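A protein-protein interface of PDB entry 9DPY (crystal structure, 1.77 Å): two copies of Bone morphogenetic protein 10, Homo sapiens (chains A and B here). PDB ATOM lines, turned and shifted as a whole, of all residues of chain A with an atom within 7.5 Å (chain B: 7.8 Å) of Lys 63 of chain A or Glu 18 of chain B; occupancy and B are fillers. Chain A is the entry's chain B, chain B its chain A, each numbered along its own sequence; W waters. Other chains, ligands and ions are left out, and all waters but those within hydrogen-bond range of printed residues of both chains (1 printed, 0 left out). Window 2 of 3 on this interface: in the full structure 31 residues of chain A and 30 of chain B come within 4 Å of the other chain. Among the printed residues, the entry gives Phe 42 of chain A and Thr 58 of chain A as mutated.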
ATOM      1  N   PHE A  42       9.627  18.484 -15.367  1.00  0.00           N
ATOM      2  CA  PHE A  42       8.745  18.299 -14.231  1.00  0.00           C
ATOM      3  C   PHE A  42       7.849  19.523 -14.057  1.00  0.00           C
ATOM      4  O   PHE A  42       8.332  20.659 -14.125  1.00  0.00           O
ATOM      5  CB  PHE A  42       9.557  18.082 -12.956  1.00  0.00           C
ATOM      6  CG  PHE A  42       8.714  17.697 -11.768  1.00  0.00           C
ATOM      7  CD1 PHE A  42       8.360  16.374 -11.554  1.00  0.00           C
ATOM      8  CD2 PHE A  42       8.255  18.663 -10.892  1.00  0.00           C
ATOM      9  CE1 PHE A  42       7.580  16.016 -10.483  1.00  0.00           C
ATOM     10  CE2 PHE A  42       7.473  18.321  -9.816  1.00  0.00           C
ATOM     11  CZ  PHE A  42       7.140  16.998  -9.605  1.00  0.00           C
ATOM     12  N   ILE A  56      10.861   9.603 -11.115  1.00  0.00           N
ATOM     13  CA  ILE A  56      11.812   9.686 -10.008  1.00  0.00           C
ATOM     14  C   ILE A  56      13.173  10.161 -10.498  1.00  0.00           C
ATOM     15  O   ILE A  56      13.864  10.923  -9.815  1.00  0.00           O
ATOM     16  CB  ILE A  56      11.920   8.328  -9.296  1.00  0.00           C
ATOM     17  CG1 ILE A  56      10.531   7.851  -8.862  1.00  0.00           C
ATOM     18  CG2 ILE A  56      12.790   8.446  -8.063  1.00  0.00           C
ATOM     19  CD1 ILE A  56      10.525   6.457  -8.335  1.00  0.00           C
ATOM     20  N   GLN A  57      13.600   9.697 -11.668  1.00  0.00           N
ATOM     21  CA  GLN A  57      14.855  10.194 -12.226  1.00  0.00           C
ATOM     22  C   GLN A  57      14.788  11.694 -12.473  1.00  0.00           C
ATOM     23  O   GLN A  57      15.740  12.432 -12.177  1.00  0.00           O
ATOM     24  CB  GLN A  57      15.161   9.438 -13.520  1.00  0.00           C
ATOM     25  CG  GLN A  57      16.500   9.774 -14.129  1.00  0.00           C
ATOM     26  CD  GLN A  57      16.722   9.044 -15.425  1.00  0.00           C
ATOM     27  OE1 GLN A  57      16.598   7.808 -15.499  1.00  0.00           O
ATOM     28  NE2 GLN A  57      17.054   9.792 -16.471  1.00  0.00           N
ATOM     29  N   THR A  58      13.666  12.169 -13.003  1.00  0.00           N
ATOM     30  CA  THR A  58      13.529  13.595 -13.254  1.00  0.00           C
ATOM     31  C   THR A  58      13.615  14.386 -11.958  1.00  0.00           C
ATOM     32  O   THR A  58      14.234  15.455 -11.918  1.00  0.00           O
ATOM     33  CB  THR A  58      12.206  13.875 -13.969  1.00  0.00           C
ATOM     34  OG1 THR A  58      12.217  13.254 -15.263  1.00  0.00           O
ATOM     35  CG2 THR A  58      11.982  15.373 -14.152  1.00  0.00           C
ATOM     36  N   LEU A  59      12.987  13.880 -10.888  1.00  0.00           N
ATOM     37  CA  LEU A  59      12.966  14.604  -9.621  1.00  0.00           C
ATOM     38  C   LEU A  59      14.339  14.623  -8.967  1.00  0.00           C
ATOM     39  O   LEU A  59      14.767  15.660  -8.445  1.00  0.00           O
ATOM     40  CB  LEU A  59      11.942  13.976  -8.668  1.00  0.00           C
ATOM     41  CG  LEU A  59      10.506  14.497  -8.803  1.00  0.00           C
ATOM     42  CD1 LEU A  59       9.565  13.707  -7.909  1.00  0.00           C
ATOM     43  CD2 LEU A  59      10.453  15.978  -8.463  1.00  0.00           C
ATOM     44  N   VAL A  60      15.043  13.490  -8.989  1.00  0.00           N
ATOM     45  CA  VAL A  60      16.413  13.453  -8.480  1.00  0.00           C
ATOM     46  C   VAL A  60      17.266  14.503  -9.180  1.00  0.00           C
ATOM     47  O   VAL A  60      18.036  15.232  -8.543  1.00  0.00           O
ATOM     48  CB  VAL A  60      17.009  12.044  -8.660  1.00  0.00           C
ATOM     49  CG1 VAL A  60      18.527  12.055  -8.525  1.00  0.00           C
ATOM     50  CG2 VAL A  60      16.420  11.065  -7.655  1.00  0.00           C
ATOM     51  N   HIS A  61      17.149  14.582 -10.513  1.00  0.00           N
ATOM     52  CA  HIS A  61      17.985  15.481 -11.308  1.00  0.00           C
ATOM     53  C   HIS A  61      17.544  16.927 -11.162  1.00  0.00           C
ATOM     54  O   HIS A  61      18.342  17.853 -11.348  1.00  0.00           O
ATOM     55  CB  HIS A  61      17.915  15.060 -12.782  1.00  0.00           C
ATOM     56  CG  HIS A  61      18.875  15.779 -13.686  1.00  0.00           C
ATOM     57  ND1 HIS A  61      20.244  15.680 -13.562  1.00  0.00           N
ATOM     58  CD2 HIS A  61      18.637  16.606 -14.709  1.00  0.00           C
ATOM     59  CE1 HIS A  61      20.815  16.422 -14.492  1.00  0.00           C
ATOM     60  NE2 HIS A  61      19.861  16.970 -15.226  1.00  0.00           N
ATOM     61  N   LEU A  62      16.274  17.135 -10.851  1.00  0.00           N
ATOM     62  CA  LEU A  62      15.747  18.488 -10.805  1.00  0.00           C
ATOM     63  C   LEU A  62      16.475  19.318  -9.759  1.00  0.00           C
ATOM     64  O   LEU A  62      16.830  20.479 -10.008  1.00  0.00           O
ATOM     65  CB  LEU A  62      14.249  18.424 -10.535  1.00  0.00           C
ATOM     66  CG  LEU A  62      13.603  19.785 -10.291  1.00  0.00           C
ATOM     67  CD1 LEU A  62      13.703  20.641 -11.549  1.00  0.00           C
ATOM     68  CD2 LEU A  62      12.160  19.626  -9.844  1.00  0.00           C
ATOM     69  N   LYS A  63      16.757  18.723  -8.604  1.00  0.00           N
ATOM     70  CA  LYS A  63      17.406  19.429  -7.510  1.00  0.00           C
ATOM     71  C   LYS A  63      18.875  19.073  -7.420  1.00  0.00           C
ATOM     72  O   LYS A  63      19.568  19.537  -6.512  1.00  0.00           O
ATOM     73  CB  LYS A  63      16.713  19.105  -6.175  1.00  0.00           C
ATOM     74  CG  LYS A  63      15.203  18.836  -6.316  1.00  0.00           C
ATOM     75  CD  LYS A  63      14.758  17.561  -5.632  1.00  0.00           C
ATOM     76  CE  LYS A  63      13.300  17.230  -5.865  1.00  0.00           C
ATOM     77  NZ  LYS A  63      12.411  18.020  -4.981  1.00  0.00           N
ATOM     78  N   ASN A  64      19.352  18.243  -8.340  1.00  0.00           N
ATOM     79  CA  ASN A  64      20.792  17.891  -8.410  1.00  0.00           C
ATOM     80  C   ASN A  64      21.091  17.664  -9.888  1.00  0.00           C
ATOM     81  O   ASN A  64      20.736  16.611 -10.427  1.00  0.00           O
ATOM     82  CB  ASN A  64      21.127  16.657  -7.569  1.00  0.00           C
ATOM     83  CG  ASN A  64      22.613  16.395  -7.439  1.00  0.00           C
ATOM     84  OD1 ASN A  64      23.411  16.821  -8.274  1.00  0.00           O
ATOM     85  ND2 ASN A  64      22.995  15.685  -6.384  1.00  0.00           N
ATOM     86  N   SER A  65      21.738  18.630 -10.542  1.00  0.00           N
ATOM     87  CA  SER A  65      22.007  18.480 -11.971  1.00  0.00           C
ATOM     88  C   SER A  65      23.238  17.623 -12.252  1.00  0.00           C
ATOM     89  O   SER A  65      23.486  17.277 -13.416  1.00  0.00           O
ATOM     90  CB  SER A  65      22.190  19.851 -12.618  1.00  0.00           C
ATOM     91  OG  SER A  65      23.461  20.365 -12.257  1.00  0.00           O
ATOM     92  N   GLN A  66      23.999  17.267 -11.217  1.00  0.00           N
ATOM     93  CA  GLN A  66      25.160  16.396 -11.336  1.00  0.00           C
ATOM     94  C   GLN A  66      24.872  14.963 -10.900  1.00  0.00           C
ATOM     95  O   GLN A  66      25.799  14.158 -10.750  1.00  0.00           O
ATOM     96  CB  GLN A  66      26.323  17.011 -10.553  1.00  0.00           C
ATOM     97  CG  GLN A  66      26.667  18.388 -11.145  1.00  0.00           C
ATOM     98  CD  GLN A  66      27.878  19.045 -10.537  1.00  0.00           C
ATOM     99  OE1 GLN A  66      28.276  20.147 -10.913  1.00  0.00           O
ATOM    100  NE2 GLN A  66      28.466  18.365  -9.581  1.00  0.00           N
ATOM    101  N   LYS A  67      23.604  14.608 -10.776  1.00  0.00           N
ATOM    102  CA  LYS A  67      23.194  13.251 -10.451  1.00  0.00           C
ATOM    103  C   LYS A  67      22.105  12.872 -11.448  1.00  0.00           C
ATOM    104  O   LYS A  67      21.185  13.661 -11.695  1.00  0.00           O
ATOM    105  CB  LYS A  67      22.732  13.155  -8.985  1.00  0.00           C
ATOM    106  CG  LYS A  67      22.338  11.740  -8.538  1.00  0.00           C
ATOM    107  CD  LYS A  67      21.963  11.690  -7.066  1.00  0.00           C
ATOM    108  CE  LYS A  67      21.561  10.283  -6.659  1.00  0.00           C
ATOM    109  NZ  LYS A  67      21.213  10.178  -5.215  1.00  0.00           N
ATOM    110  N   LEU B  12      22.453   3.625  -9.832  1.00  0.00           N
ATOM    111  CA  LEU B  12      21.834   4.871  -9.381  1.00  0.00           C
ATOM    112  C   LEU B  12      21.030   4.539  -8.127  1.00  0.00           C
ATOM    113  O   LEU B  12      20.001   3.864  -8.215  1.00  0.00           O
ATOM    114  CB  LEU B  12      20.957   5.470 -10.474  1.00  0.00           C
ATOM    115  CG  LEU B  12      20.274   6.788 -10.082  1.00  0.00           C
ATOM    116  CD1 LEU B  12      21.309   7.885  -9.904  1.00  0.00           C
ATOM    117  CD2 LEU B  12      19.233   7.194 -11.109  1.00  0.00           C
ATOM    118  N   TYR B  13      21.543   4.942  -6.961  1.00  0.00           N
ATOM    119  CA  TYR B  13      20.826   4.760  -5.708  1.00  0.00           C
ATOM    120  C   TYR B  13      20.031   6.027  -5.429  1.00  0.00           C
ATOM    121  O   TYR B  13      20.563   7.139  -5.547  1.00  0.00           O
ATOM    122  CB  TYR B  13      21.760   4.462  -4.532  1.00  0.00           C
ATOM    123  CG  TYR B  13      20.978   4.209  -3.243  1.00  0.00           C
ATOM    124  CD1 TYR B  13      20.457   2.951  -2.964  1.00  0.00           C
ATOM    125  CD2 TYR B  13      20.726   5.240  -2.342  1.00  0.00           C
ATOM    126  CE1 TYR B  13      19.725   2.714  -1.803  1.00  0.00           C
ATOM    127  CE2 TYR B  13      19.988   5.017  -1.174  1.00  0.00           C
ATOM    128  CZ  TYR B  13      19.495   3.751  -0.914  1.00  0.00           C
ATOM    129  OH  TYR B  13      18.770   3.504   0.225  1.00  0.00           O
ATOM    130  N   ILE B  14      18.762   5.857  -5.080  1.00  0.00           N
ATOM    131  CA  ILE B  14      17.861   6.964  -4.799  1.00  0.00           C
ATOM    132  C   ILE B  14      17.385   6.831  -3.355  1.00  0.00           C
ATOM    133  O   ILE B  14      16.702   5.862  -2.994  1.00  0.00           O
ATOM    134  CB  ILE B  14      16.685   7.011  -5.779  1.00  0.00           C
ATOM    135  CG1 ILE B  14      17.236   7.234  -7.194  1.00  0.00           C
ATOM    136  CG2 ILE B  14      15.718   8.117  -5.394  1.00  0.00           C
ATOM    137  CD1 ILE B  14      16.193   7.573  -8.218  1.00  0.00           C
ATOM    138  N   ASP B  15      17.784   7.785  -2.527  1.00  0.00           N
ATOM    139  CA  ASP B  15      17.221   7.966  -1.200  1.00  0.00           C
ATOM    140  C   ASP B  15      15.915   8.738  -1.341  1.00  0.00           C
ATOM    141  O   ASP B  15      15.889   9.813  -1.947  1.00  0.00           O
ATOM    142  CB  ASP B  15      18.222   8.735  -0.328  1.00  0.00           C
ATOM    143  CG  ASP B  15      17.867   8.702   1.150  1.00  0.00           C
ATOM    144  OD1 ASP B  15      16.715   9.022   1.496  1.00  0.00           O
ATOM    145  OD2 ASP B  15      18.746   8.344   1.959  1.00  0.00           O
ATOM    146  N   PHE B  16      14.826   8.202  -0.783  1.00  0.00           N
ATOM    147  CA  PHE B  16      13.540   8.876  -0.954  1.00  0.00           C
ATOM    148  C   PHE B  16      13.509  10.240  -0.277  1.00  0.00           C
ATOM    149  O   PHE B  16      12.707  11.096  -0.670  1.00  0.00           O
ATOM    150  CB  PHE B  16      12.403   7.978  -0.444  1.00  0.00           C
ATOM    151  CG  PHE B  16      12.099   6.816  -1.386  1.00  0.00           C
ATOM    152  CD1 PHE B  16      11.952   7.031  -2.750  1.00  0.00           C
ATOM    153  CD2 PHE B  16      12.014   5.516  -0.908  1.00  0.00           C
ATOM    154  CE1 PHE B  16      11.700   5.971  -3.619  1.00  0.00           C
ATOM    155  CE2 PHE B  16      11.765   4.475  -1.748  1.00  0.00           C
ATOM    156  CZ  PHE B  16      11.608   4.694  -3.122  1.00  0.00           C
ATOM    157  N   LYS B  17      14.368  10.476   0.710  1.00  0.00           N
ATOM    158  CA  LYS B  17      14.384  11.788   1.348  1.00  0.00           C
ATOM    159  C   LYS B  17      14.820  12.858   0.364  1.00  0.00           C
ATOM    160  O   LYS B  17      14.245  13.951   0.325  1.00  0.00           O
ATOM    161  CB  LYS B  17      15.316  11.795   2.563  1.00  0.00           C
ATOM    162  CG  LYS B  17      14.880  10.894   3.715  1.00  0.00           C
ATOM    163  CD  LYS B  17      15.759  11.125   4.942  1.00  0.00           C
ATOM    164  CE  LYS B  17      15.811   9.897   5.836  1.00  0.00           C
ATOM    165  NZ  LYS B  17      14.509   9.590   6.519  1.00  0.00           N
ATOM    166  N   GLU B  18      15.829  12.550  -0.451  1.00  0.00           N
ATOM    167  CA  GLU B  18      16.396  13.546  -1.343  1.00  0.00           C
ATOM    168  C   GLU B  18      15.405  14.029  -2.392  1.00  0.00           C
ATOM    169  O   GLU B  18      15.701  14.999  -3.097  1.00  0.00           O
ATOM    170  CB  GLU B  18      17.654  12.979  -2.026  1.00  0.00           C
ATOM    171  CG  GLU B  18      17.381  12.241  -3.341  1.00  0.00           C
ATOM    172  CD  GLU B  18      18.611  11.532  -3.879  1.00  0.00           C
ATOM    173  OE1 GLU B  18      19.140  10.643  -3.179  1.00  0.00           O
ATOM    174  OE2 GLU B  18      19.053  11.868  -4.997  1.00  0.00           O
ATOM    175  N   ILE B  19      14.251  13.380  -2.531  1.00  0.00           N
ATOM    176  CA  ILE B  19      13.210  13.841  -3.442  1.00  0.00           C
ATOM    177  C   ILE B  19      11.936  14.225  -2.710  1.00  0.00           C
ATOM    178  O   ILE B  19      10.950  14.602  -3.356  1.00  0.00           O
ATOM    179  CB  ILE B  19      12.908  12.797  -4.535  1.00  0.00           C
ATOM    180  CG1 ILE B  19      12.604  11.430  -3.917  1.00  0.00           C
ATOM    181  CG2 ILE B  19      14.082  12.691  -5.507  1.00  0.00           C
ATOM    182  CD1 ILE B  19      12.294  10.348  -4.929  1.00  0.00           C
ATOM    183  N   GLY B  20      11.932  14.153  -1.386  1.00  0.00           N
ATOM    184  CA  GLY B  20      10.765  14.472  -0.588  1.00  0.00           C
ATOM    185  C   GLY B  20       9.692  13.406  -0.570  1.00  0.00           C
ATOM    186  O   GLY B  20       8.609  13.653  -0.029  1.00  0.00           O
ATOM    187  N   TRP B  21       9.947  12.227  -1.146  1.00  0.00           N
ATOM    188  CA  TRP B  21       8.952  11.167  -1.101  1.00  0.00           C
ATOM    189  C   TRP B  21       8.896  10.464   0.246  1.00  0.00           C
ATOM    190  O   TRP B  21       8.010   9.624   0.444  1.00  0.00           O
ATOM    191  CB  TRP B  21       9.198  10.139  -2.204  1.00  0.00           C
ATOM    192  CG  TRP B  21       8.702  10.644  -3.522  1.00  0.00           C
ATOM    193  CD1 TRP B  21       8.399  11.944  -3.839  1.00  0.00           C
ATOM    194  CD2 TRP B  21       8.434   9.874  -4.694  1.00  0.00           C
ATOM    195  NE1 TRP B  21       7.948  12.021  -5.129  1.00  0.00           N
ATOM    196  CE2 TRP B  21       7.972  10.769  -5.685  1.00  0.00           C
ATOM    197  CE3 TRP B  21       8.538   8.517  -5.008  1.00  0.00           C
ATOM    198  CZ2 TRP B  21       7.620  10.349  -6.963  1.00  0.00           C
ATOM    199  CZ3 TRP B  21       8.179   8.099  -6.283  1.00  0.00           C
ATOM    200  CH2 TRP B  21       7.724   9.013  -7.242  1.00  0.00           C
ATOM    201  N   ASP B  22       9.817  10.764   1.162  1.00  0.00           N
ATOM    202  CA  ASP B  22       9.653  10.250   2.521  1.00  0.00           C
ATOM    203  C   ASP B  22       8.394  10.778   3.202  1.00  0.00           C
ATOM    204  O   ASP B  22       8.075  10.332   4.305  1.00  0.00           O
ATOM    205  CB  ASP B  22      10.863  10.606   3.373  1.00  0.00           C
ATOM    206  CG  ASP B  22      11.065  12.106   3.499  1.00  0.00           C
ATOM    207  OD1 ASP B  22      10.774  12.839   2.522  1.00  0.00           O
ATOM    208  OD2 ASP B  22      11.516  12.538   4.579  1.00  0.00           O
ATOM    209  N   PRO B  29      13.928   3.130   2.883  1.00  0.00           N
ATOM    210  CA  PRO B  29      14.421   4.523   2.797  1.00  0.00           C
ATOM    211  C   PRO B  29      14.922   4.912   1.411  1.00  0.00           C
ATOM    212  O   PRO B  29      14.940   6.102   1.068  1.00  0.00           O
ATOM    213  CB  PRO B  29      15.565   4.552   3.821  1.00  0.00           C
ATOM    214  CG  PRO B  29      16.007   3.117   3.937  1.00  0.00           C
ATOM    215  CD  PRO B  29      14.751   2.298   3.780  1.00  0.00           C
ATOM    216  N   GLY B  30      15.357   3.940   0.623  1.00  0.00           N
ATOM    217  CA  GLY B  30      15.866   4.190  -0.713  1.00  0.00           C
ATOM    218  C   GLY B  30      15.966   2.861  -1.428  1.00  0.00           C
ATOM    219  O   GLY B  30      15.667   1.808  -0.860  1.00  0.00           O
HETATM  220  O   HOH W   1      18.785  15.009  -5.526  1.00  0.00           O
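The side-chain carboxylate of Glu 18 of chain B lies within salt-bridge range of the side-chain amino group of Lys 67 of chain A (2.8 Å). The backbone carbonyl oxygen of Tyr 13 of chain B sits at hydrogen-bond distance from the side-chain amino group of Lys 67 of chain A (3.1 Å).
The backbone carbonyl oxygen of Lys 67 of chain A lies within hydrogen-bond range of a ring nitrogen (ND1) of His 61 of chain A, at 2.9 Å. The side-chain carboxylate (OE1) of Glu 18 of chain B sits at hydrogen-bond distance from the backbone NH (N) of Asp 15 of chain B, at 3.2 Å. The backbone NH of Gly 30 of chain B lies close to the side-chain hydroxyl of Tyr 13 of chain B, at 3.5 Å. OD1 of Asn 64 of chain A sits at hydrogen-bond distance from N of Lys 67 of chain A (3.3 Å). N of Trp 21 of chain B sits at hydrogen-bond distance from O of Phe 16 of chain B.
Among the printed residues, pairs that only touch across the chains: Ile 56 of chain A with Ile 14 of chain B, Ile 56 of chain A with Ile 19 of chain B, Ile 56 of chain A with Trp 21 of chain B, Leu 59 of chain A with Ile 19 of chain B, Leu 59 of chain A with Trp 21 of chain B, Val 60 of chain A with Ile 14 of chain B, Val 60 of chain A with Glu 18 of chain B, Val 60 of chain A with Ile 19 of chain B and Lys 63 of chain A with Glu 18 of chain B.
Of chain B, only Glu 18 (3.7 Å) comes within 4 Å of Lys 63 of chain A. Glu 18 of chain B touches just these residues of chain A: Val 60 (3.6 Å), Lys 63 (3.7 Å) and Lys 67 (2.8 Å). Of the printed residues of chain A, Ile 19 of chain B touches Ile 56, Leu 59 and Val 60. Printed residues of chain B within 4 Å of Leu 59 of chain A: Ile 19 (3.97 Å) and Trp 21 (3.6 Å). Printed residues of chain A within 4 Å of Tyr 13 of chain B: Lys 67. Of the printed residues of chain A, Trp 21 of chain B touches Ile 56 and Leu 59. Gly 20 of chain B touches none of the printed residues of chain A. Asp 15 of chain B touches none of the printed residues of chain A. The nearest residue of chain A that does not touch Glu 18 of chain B is Leu 59 of chain A (5.5 Å). The nearest printed residue of chain A that does not touch Trp 21 of chain B is Phe 42 of chain A (6.7 Å).
Printed residues of chain A that touch a printed residue of chain B: Ile 56, Leu 59, Val 60, Lys 63 and Lys 67. Hydrophobic or aromatic side chains of chain B that line the printed part of chain A: Ile 14, Ile 19 and Trp 21. Among the printed residues, 11 pairs touch across the chains.
No position is printed for both chains.
Water W1 bridges O of Val 60 of chain A (3.1 Å) and OE2 of Glu 18 of chain B (3.2 Å).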
